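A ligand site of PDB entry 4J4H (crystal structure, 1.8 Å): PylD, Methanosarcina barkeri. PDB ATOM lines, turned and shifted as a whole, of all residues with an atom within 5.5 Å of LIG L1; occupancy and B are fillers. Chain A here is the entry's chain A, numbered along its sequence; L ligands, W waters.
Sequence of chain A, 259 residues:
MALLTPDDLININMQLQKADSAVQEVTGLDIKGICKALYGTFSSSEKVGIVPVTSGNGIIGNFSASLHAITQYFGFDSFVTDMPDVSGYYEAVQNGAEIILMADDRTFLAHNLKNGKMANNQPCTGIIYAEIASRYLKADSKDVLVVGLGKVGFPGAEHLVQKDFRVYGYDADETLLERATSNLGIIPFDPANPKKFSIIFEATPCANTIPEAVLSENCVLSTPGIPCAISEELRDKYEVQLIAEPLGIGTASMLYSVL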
ATOM      1  N   ALA A   2     -19.835  20.081  17.393  1.00  0.00           N
ATOM      2  CA  ALA A   2     -19.028  20.827  18.348  1.00  0.00           C
ATOM      3  C   ALA A   2     -19.877  21.259  19.539  1.00  0.00           C
ATOM      4  O   ALA A   2     -20.758  22.112  19.416  1.00  0.00           O
ATOM      5  CB  ALA A   2     -18.388  22.036  17.671  1.00  0.00           C
ATOM      6  N   LEU A   3     -19.618  20.639  20.690  1.00  0.00           N
ATOM      7  CA  LEU A   3     -20.434  20.859  21.879  1.00  0.00           C
ATOM      8  C   LEU A   3     -19.777  21.789  22.895  1.00  0.00           C
ATOM      9  O   LEU A   3     -18.554  21.955  22.905  1.00  0.00           O
ATOM     10  CB  LEU A   3     -20.786  19.526  22.559  1.00  0.00           C
ATOM     11  CG  LEU A   3     -21.387  18.409  21.696  1.00  0.00           C
ATOM     12  CD1 LEU A   3     -21.709  17.204  22.562  1.00  0.00           C
ATOM     13  CD2 LEU A   3     -22.626  18.876  20.948  1.00  0.00           C
ATOM     14  N   LEU A   4     -20.603  22.393  23.740  1.00  0.00           N
ATOM     15  CA  LEU A   4     -20.144  23.237  24.831  1.00  0.00           C
ATOM     16  C   LEU A   4     -19.238  22.486  25.809  1.00  0.00           C
ATOM     17  O   LEU A   4     -19.431  21.296  26.059  1.00  0.00           O
ATOM     18  CB  LEU A   4     -21.331  23.796  25.615  1.00  0.00           C
ATOM     19  CG  LEU A   4     -22.162  24.900  24.961  1.00  0.00           C
ATOM     20  CD1 LEU A   4     -23.377  25.182  25.820  1.00  0.00           C
ATOM     21  CD2 LEU A   4     -21.330  26.155  24.771  1.00  0.00           C
ATOM     22  N   VAL A  51     -34.039  19.170  32.451  1.00  0.00           N
ATOM     23  CA  VAL A  51     -33.738  17.753  32.649  1.00  0.00           C
ATOM     24  C   VAL A  51     -32.329  17.425  32.151  1.00  0.00           C
ATOM     25  O   VAL A  51     -32.069  17.487  30.943  1.00  0.00           O
ATOM     26  CB  VAL A  51     -34.760  16.852  31.928  1.00  0.00           C
ATOM     27  CG1 VAL A  51     -34.433  15.385  32.151  1.00  0.00           C
ATOM     28  CG2 VAL A  51     -36.179  17.140  32.418  1.00  0.00           C
ATOM     29  N   PRO A  52     -31.415  17.068  33.081  1.00  0.00           N
ATOM     30  CA  PRO A  52     -30.073  16.654  32.638  1.00  0.00           C
ATOM     31  C   PRO A  52     -30.167  15.347  31.845  1.00  0.00           C
ATOM     32  O   PRO A  52     -31.016  14.504  32.132  1.00  0.00           O
ATOM     33  CB  PRO A  52     -29.314  16.440  33.951  1.00  0.00           C
ATOM     34  CG  PRO A  52     -30.113  17.168  34.992  1.00  0.00           C
ATOM     35  CD  PRO A  52     -31.540  17.009  34.545  1.00  0.00           C
ATOM     36  N   VAL A  53     -29.300  15.209  30.843  1.00  0.00           N
ATOM     37  CA  VAL A  53     -29.350  14.054  29.944  1.00  0.00           C
ATOM     38  C   VAL A  53     -27.955  13.411  29.818  1.00  0.00           C
ATOM     39  O   VAL A  53     -26.973  14.088  29.494  1.00  0.00           O
ATOM     40  CB  VAL A  53     -29.931  14.441  28.549  1.00  0.00           C
ATOM     41  CG1 VAL A  53     -29.742  13.329  27.529  1.00  0.00           C
ATOM     42  CG2 VAL A  53     -31.408  14.808  28.661  1.00  0.00           C
ATOM     43  N   THR A  54     -27.889  12.107  30.075  1.00  0.00           N
ATOM     44  CA  THR A  54     -26.617  11.372  30.106  1.00  0.00           C
ATOM     45  C   THR A  54     -26.268  10.743  28.754  1.00  0.00           C
ATOM     46  O   THR A  54     -25.239  10.063  28.625  1.00  0.00           O
ATOM     47  CB  THR A  54     -26.601  10.273  31.185  1.00  0.00           C
ATOM     48  OG1 THR A  54     -27.548   9.244  30.852  1.00  0.00           O
ATOM     49  CG2 THR A  54     -26.927  10.848  32.570  1.00  0.00           C
ATOM     50  N   SER A  55     -27.115  10.971  27.754  1.00  0.00           N
ATOM     51  CA  SER A  55     -26.949  10.429  26.401  1.00  0.00           C
ATOM     52  C   SER A  55     -25.637  10.852  25.727  1.00  0.00           C
ATOM     53  O   SER A  55     -25.158  11.964  25.951  1.00  0.00           O
ATOM     54  CB  SER A  55     -28.146  10.838  25.545  1.00  0.00           C
ATOM     55  OG  SER A  55     -27.886  10.704  24.158  1.00  0.00           O
ATOM     56  N   GLY A  58     -22.645  12.644  27.280  1.00  0.00           N
ATOM     57  CA  GLY A  58     -23.142  12.699  28.649  1.00  0.00           C
ATOM     58  C   GLY A  58     -23.371  14.102  29.188  1.00  0.00           C
ATOM     59  O   GLY A  58     -23.369  15.073  28.429  1.00  0.00           O
ATOM     60  N   ILE A  59     -23.578  14.182  30.493  1.00  0.00           N
ATOM     61  CA  ILE A  59     -23.809  15.456  31.174  1.00  0.00           C
ATOM     62  C   ILE A  59     -22.579  16.361  31.031  1.00  0.00           C
ATOM     63  O   ILE A  59     -21.449  15.917  31.236  1.00  0.00           O
ATOM     64  CB  ILE A  59     -24.184  15.243  32.655  1.00  0.00           C
ATOM     65  CG1 ILE A  59     -25.590  14.614  32.760  1.00  0.00           C
ATOM     66  CG2 ILE A  59     -24.129  16.561  33.438  1.00  0.00           C
ATOM     67  CD1 ILE A  59     -25.999  14.171  34.151  1.00  0.00           C
ATOM     68  N   ILE A  60     -22.830  17.605  30.637  1.00  0.00           N
ATOM     69  CA  ILE A  60     -21.769  18.604  30.513  1.00  0.00           C
ATOM     70  C   ILE A  60     -21.750  19.455  31.781  1.00  0.00           C
ATOM     71  O   ILE A  60     -22.782  20.016  32.170  1.00  0.00           O
ATOM     72  CB  ILE A  60     -21.965  19.498  29.264  1.00  0.00           C
ATOM     73  CG1 ILE A  60     -21.898  18.651  27.983  1.00  0.00           C
ATOM     74  CG2 ILE A  60     -20.940  20.628  29.245  1.00  0.00           C
ATOM     75  CD1 ILE A  60     -22.156  19.426  26.711  1.00  0.00           C
ATOM     76  N   PHE A  63     -23.763  22.875  32.505  1.00  0.00           N
ATOM     77  CA  PHE A  63     -24.845  23.018  31.520  1.00  0.00           C
ATOM     78  C   PHE A  63     -26.216  23.288  32.157  1.00  0.00           C
ATOM     79  O   PHE A  63     -26.811  24.327  31.906  1.00  0.00           O
ATOM     80  CB  PHE A  63     -24.908  21.820  30.554  1.00  0.00           C
ATOM     81  CG  PHE A  63     -25.902  21.998  29.433  1.00  0.00           C
ATOM     82  CD1 PHE A  63     -25.612  22.835  28.345  1.00  0.00           C
ATOM     83  CD2 PHE A  63     -27.126  21.342  29.459  1.00  0.00           C
ATOM     84  CE1 PHE A  63     -26.522  23.006  27.321  1.00  0.00           C
ATOM     85  CE2 PHE A  63     -28.041  21.500  28.418  1.00  0.00           C
ATOM     86  CZ  PHE A  63     -27.736  22.328  27.354  1.00  0.00           C
ATOM     87  N   SER A  64     -26.701  22.358  32.978  1.00  0.00           N
ATOM     88  CA  SER A  64     -28.016  22.545  33.627  1.00  0.00           C
ATOM     89  C   SER A  64     -28.024  23.753  34.570  1.00  0.00           C
ATOM     90  O   SER A  64     -29.026  24.465  34.643  1.00  0.00           O
ATOM     91  CB  SER A  64     -28.455  21.285  34.382  1.00  0.00           C
ATOM     92  OG  SER A  64     -27.620  21.046  35.499  1.00  0.00           O
ATOM     93  N   ALA A 103     -31.447  18.513  26.450  1.00  0.00           N
ATOM     94  CA  ALA A 103     -30.558  18.395  25.305  1.00  0.00           C
ATOM     95  C   ALA A 103     -29.773  17.090  25.319  1.00  0.00           C
ATOM     96  O   ALA A 103     -29.275  16.682  26.358  1.00  0.00           O
ATOM     97  CB  ALA A 103     -29.583  19.557  25.269  1.00  0.00           C
ATOM     98  N   ASP A 104     -29.692  16.429  24.161  1.00  0.00           N
ATOM     99  CA  ASP A 104     -28.654  15.427  23.933  1.00  0.00           C
ATOM    100  C   ASP A 104     -27.589  16.042  23.014  1.00  0.00           C
ATOM    101  O   ASP A 104     -27.588  17.256  22.815  1.00  0.00           O
ATOM    102  CB  ASP A 104     -29.220  14.066  23.454  1.00  0.00           C
ATOM    103  CG  ASP A 104     -29.926  14.129  22.079  1.00  0.00           C
ATOM    104  OD1 ASP A 104     -29.665  15.034  21.267  1.00  0.00           O
ATOM    105  OD2 ASP A 104     -30.742  13.210  21.814  1.00  0.00           O
ATOM    106  N   ASP A 105     -26.687  15.228  22.478  1.00  0.00           N
ATOM    107  CA  ASP A 105     -25.581  15.758  21.654  1.00  0.00           C
ATOM    108  C   ASP A 105     -26.042  16.359  20.330  1.00  0.00           C
ATOM    109  O   ASP A 105     -25.333  17.177  19.742  1.00  0.00           O
ATOM    110  CB  ASP A 105     -24.533  14.660  21.393  1.00  0.00           C
ATOM    111  CG  ASP A 105     -23.756  14.273  22.646  1.00  0.00           C
ATOM    112  OD1 ASP A 105     -23.968  14.865  23.728  1.00  0.00           O
ATOM    113  OD2 ASP A 105     -22.913  13.352  22.547  1.00  0.00           O
ATOM    114  N   PHE A 108     -31.180  20.129  21.157  1.00  0.00           N
ATOM    115  CA  PHE A 108     -31.489  20.870  22.363  1.00  0.00           C
ATOM    116  C   PHE A 108     -32.852  21.486  22.115  1.00  0.00           C
ATOM    117  O   PHE A 108     -33.029  22.297  21.194  1.00  0.00           O
ATOM    118  CB  PHE A 108     -30.378  21.907  22.636  1.00  0.00           C
ATOM    119  CG  PHE A 108     -30.670  22.886  23.759  1.00  0.00           C
ATOM    120  CD1 PHE A 108     -31.535  22.563  24.809  1.00  0.00           C
ATOM    121  CD2 PHE A 108     -30.032  24.122  23.784  1.00  0.00           C
ATOM    122  CE1 PHE A 108     -31.770  23.470  25.835  1.00  0.00           C
ATOM    123  CE2 PHE A 108     -30.272  25.038  24.800  1.00  0.00           C
ATOM    124  CZ  PHE A 108     -31.147  24.715  25.836  1.00  0.00           C
ATOM    125  N   ASN A 121     -32.949  24.342  19.257  1.00  0.00           N
ATOM    126  CA  ASN A 121     -31.909  25.332  19.519  1.00  0.00           C
ATOM    127  C   ASN A 121     -31.212  25.879  18.277  1.00  0.00           C
ATOM    128  O   ASN A 121     -30.850  27.059  18.234  1.00  0.00           O
ATOM    129  CB  ASN A 121     -30.858  24.751  20.471  1.00  0.00           C
ATOM    130  CG  ASN A 121     -29.723  25.713  20.769  1.00  0.00           C
ATOM    131  OD1 ASN A 121     -28.607  25.521  20.271  1.00  0.00           O
ATOM    132  ND2 ASN A 121     -29.995  26.752  21.547  1.00  0.00           N
ATOM    133  N   PRO A 246     -22.385  32.055  24.872  1.00  0.00           N
ATOM    134  CA  PRO A 246     -22.346  30.611  24.588  1.00  0.00           C
ATOM    135  C   PRO A 246     -23.669  29.825  24.640  1.00  0.00           C
ATOM    136  O   PRO A 246     -23.722  28.722  24.089  1.00  0.00           O
ATOM    137  CB  PRO A 246     -21.401  30.082  25.667  1.00  0.00           C
ATOM    138  CG  PRO A 246     -21.601  31.004  26.814  1.00  0.00           C
ATOM    139  CD  PRO A 246     -21.797  32.364  26.189  1.00  0.00           C
ATOM    140  N   LEU A 247     -24.706  30.348  25.296  1.00  0.00           N
ATOM    141  CA  LEU A 247     -25.923  29.557  25.533  1.00  0.00           C
ATOM    142  C   LEU A 247     -27.204  30.386  25.740  1.00  0.00           C
ATOM    143  O   LEU A 247     -28.282  29.998  25.277  1.00  0.00           O
ATOM    144  CB  LEU A 247     -25.718  28.603  26.728  1.00  0.00           C
ATOM    145  CG  LEU A 247     -26.780  27.570  27.111  1.00  0.00           C
ATOM    146  CD1 LEU A 247     -27.071  26.581  25.982  1.00  0.00           C
ATOM    147  CD2 LEU A 247     -26.357  26.821  28.376  1.00  0.00           C
HETATM  148  C1  LIG L   1     -25.512  18.392  25.964  1.00  0.00           C
HETATM  149  C2  LIG L   1     -25.673  19.684  25.167  1.00  0.00           C
HETATM  150  C3  LIG L   1     -24.858  19.660  23.872  1.00  0.00           C
HETATM  151  C4  LIG L   1     -24.650  21.801  22.781  1.00  0.00           C
HETATM  152  C5  LIG L   1     -25.602  25.243  22.717  1.00  0.00           C
HETATM  153  O1  LIG L   1     -27.738  17.425  29.925  1.00  0.00           O
HETATM  154  C6  LIG L   1     -26.541  17.661  29.612  1.00  0.00           C
HETATM  155  O2  LIG L   1     -25.722  18.177  30.414  1.00  0.00           O
HETATM  156  C7  LIG L   1     -26.057  17.326  28.220  1.00  0.00           C
HETATM  157  N1  LIG L   1     -26.829  16.204  27.621  1.00  0.00           N
HETATM  158  C8  LIG L   1     -26.125  18.573  27.339  1.00  0.00           C
HETATM  159  N2  LIG L   1     -25.403  20.656  22.930  1.00  0.00           N
HETATM  160  O3  LIG L   1     -23.523  21.921  23.238  1.00  0.00           O
HETATM  161  C9  LIG L   1     -25.273  22.934  22.012  1.00  0.00           C
HETATM  162  C10 LIG L   1     -26.064  23.823  22.981  1.00  0.00           C
HETATM  163  C11 LIG L   1     -24.300  25.121  21.941  1.00  0.00           C
HETATM  164  N3  LIG L   1     -24.245  23.770  21.369  1.00  0.00           N
HETATM  165  P1  LG2 L   2     -22.392  23.144  11.742  1.00  0.00           P
HETATM  166  O1  LG2 L   2     -21.201  22.213  11.746  1.00  0.00           O
HETATM  167  O2  LG2 L   2     -23.761  22.608  11.431  1.00  0.00           O
HETATM  168  O3  LG2 L   2     -22.071  24.381  10.775  1.00  0.00           O
HETATM  169  C1  LG2 L   2     -20.798  25.010  10.779  1.00  0.00           C
HETATM  170  C2  LG2 L   2     -20.448  25.379   9.349  1.00  0.00           C
HETATM  171  O4  LG2 L   2     -19.355  26.293   9.306  1.00  0.00           O
HETATM  172  C3  LG2 L   2     -20.046  24.162   8.516  1.00  0.00           C
HETATM  173  O5  LG2 L   2     -20.911  24.090   7.380  1.00  0.00           O
HETATM  174  C4  LG2 L   2     -18.621  24.442   8.089  1.00  0.00           C
HETATM  175  O6  LG2 L   2     -18.334  24.001   6.764  1.00  0.00           O
HETATM  176  C5  LG2 L   2     -18.542  25.962   8.186  1.00  0.00           C
HETATM  177  N1  LG2 L   2     -17.166  26.481   8.323  1.00  0.00           N
HETATM  178  C6  LG2 L   2     -16.158  25.968   9.057  1.00  0.00           C
HETATM  179  N2  LG2 L   2     -15.034  26.728   8.932  1.00  0.00           N
HETATM  180  C7  LG2 L   2     -15.320  27.742   8.094  1.00  0.00           C
HETATM  181  C8  LG2 L   2     -14.595  28.903   7.521  1.00  0.00           C
HETATM  182  N3  LG2 L   2     -13.298  29.141   7.826  1.00  0.00           N
HETATM  183  N4  LG2 L   2     -15.268  29.722   6.690  1.00  0.00           N
HETATM  184  C9  LG2 L   2     -16.556  29.515   6.367  1.00  0.00           C
HETATM  185  N5  LG2 L   2     -17.276  28.481   6.843  1.00  0.00           N
HETATM  186  C10 LG2 L   2     -16.723  27.579   7.699  1.00  0.00           C
HETATM  187  O7  LG2 L   2     -22.395  23.841  13.193  1.00  0.00           O
HETATM  188  P2  LG2 L   2     -23.686  24.567  13.833  1.00  0.00           P
HETATM  189  O8  LG2 L   2     -24.564  23.516  14.448  1.00  0.00           O
HETATM  190  O9  LG2 L   2     -24.261  25.534  12.834  1.00  0.00           O
HETATM  191  O10 LG2 L   2     -22.997  25.400  15.039  1.00  0.00           O
HETATM  192  C11 LG2 L   2     -21.988  26.373  14.783  1.00  0.00           C
HETATM  193  C12 LG2 L   2     -21.255  26.787  16.058  1.00  0.00           C
HETATM  194  O11 LG2 L   2     -22.141  27.392  16.996  1.00  0.00           O
HETATM  195  C13 LG2 L   2     -20.595  25.633  16.811  1.00  0.00           C
HETATM  196  O12 LG2 L   2     -19.333  26.140  17.264  1.00  0.00           O
HETATM  197  C14 LG2 L   2     -21.477  25.384  18.009  1.00  0.00           C
HETATM  198  O13 LG2 L   2     -20.702  24.887  19.106  1.00  0.00           O
HETATM  199  C15 LG2 L   2     -22.017  26.778  18.292  1.00  0.00           C
HETATM  200  N6  LG2 L   2     -23.340  26.914  18.884  1.00  0.00           N
HETATM  201  C16 LG2 L   2     -23.493  27.969  19.691  1.00  0.00           C
HETATM  202  C17 LG2 L   2     -24.692  28.276  20.316  1.00  0.00           C
HETATM  203  C18 LG2 L   2     -24.748  29.485  21.208  1.00  0.00           C
HETATM  204  O14 LG2 L   2     -25.782  29.747  21.798  1.00  0.00           O
HETATM  205  N7  LG2 L   2     -23.670  30.267  21.301  1.00  0.00           N
HETATM  206  C19 LG2 L   2     -25.914  27.417  20.060  1.00  0.00           C
HETATM  207  C20 LG2 L   2     -25.628  26.301  19.142  1.00  0.00           C
HETATM  208  C21 LG2 L   2     -24.368  26.102  18.582  1.00  0.00           C
HETATM  209  O   HOH W   1     -26.953  19.011  32.663  1.00  0.00           O
HETATM  210  O   HOH W   2     -21.306  24.358  21.582  1.00  0.00           O
HETATM  211  O   HOH W   3     -30.196  18.414  29.152  1.00  0.00           O
HETATM  212  O   HOH W   4     -27.644  19.863  21.819  1.00  0.00           O
HETATM  213  O   HOH W   5     -25.957  14.547  25.701  1.00  0.00           O
HETATM  214  O   HOH W   6     -23.876  21.969  18.978  1.00  0.00           O
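O of Pro 246 sits close to N7 of LG2 L2 (3.2 Å). N of Ile 60 sits at hydrogen-bond distance from O2 of LIG L1 (3.0 Å). O of Ala 2 lies within hydrogen-bond range of O13 of LG2 L2 (2.8 Å). N of Leu 4 sits at hydrogen-bond distance from O3 of LIG L1, 3.0 Å away. O1 of LIG L1 is in hydrogen-bond range of N of Val 53 (2.9 Å). The backbone carbonyl oxygen of Val 53 is in hydrogen-bond range of a nitrogen (N1) of LIG L1. O of Ala 103 lies within hydrogen-bond range of N1 of LIG L1 (2.8 Å).
The backbone NH (N) of Asn 121 is in hydrogen-bond range of the backbone carbonyl oxygen (O) of Phe 108, 2.8 Å away.
Merely in contact with LIG L1: Leu 3 (3.5 Å), Pro 52 (3.7 Å), Gly 58 (3.5 Å), Ile 59 (3.4 Å), Phe 63 (3.6 Å), Asp 104 (3.8 Å), Asn 121 (3.9 Å) and Leu 247 (3.8 Å). Hydrophobic or aromatic side chains that line LIG L1: Leu 3, Leu 4, Val 53, Ile 59, Ile 60, Phe 63, Ala 103 and Leu 247. Of the 20 residues printed, 12 come within 4 Å of LIG L1. The nearest printed residue that does not touch LIG L1 is Phe 108 (4.1 Å).
Water W4 lies within hydrogen-bond range of N2 of LIG L1 and O of Asp 104. Water W5 lies within hydrogen-bond range of N1 of LIG L1, O of Ser 55 and OD1 of Asp 105. Water W1 lies within hydrogen-bond range of O2 of LIG L1 and N of Ser 64. Water W3 lies within hydrogen-bond range of O of Val 51 (2.8 Å), O1 of LIG L1 (2.8 Å) and N of Ala 103 (3.0 Å). Water W2 lies within hydrogen-bond range of an oxygen (O13) of LG2 L2 (2.6 Å), the backbone NH (N) of Leu 4 (3.0 Å), a nitrogen (N3) of LIG L1 (3.0 Å) and the backbone carbonyl oxygen (O) of Ala 2 (3.2 Å). Water W6 lies within hydrogen-bond range of N3 of LIG L1 (3.0 Å) and O of Ala 2 (3.2 Å).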
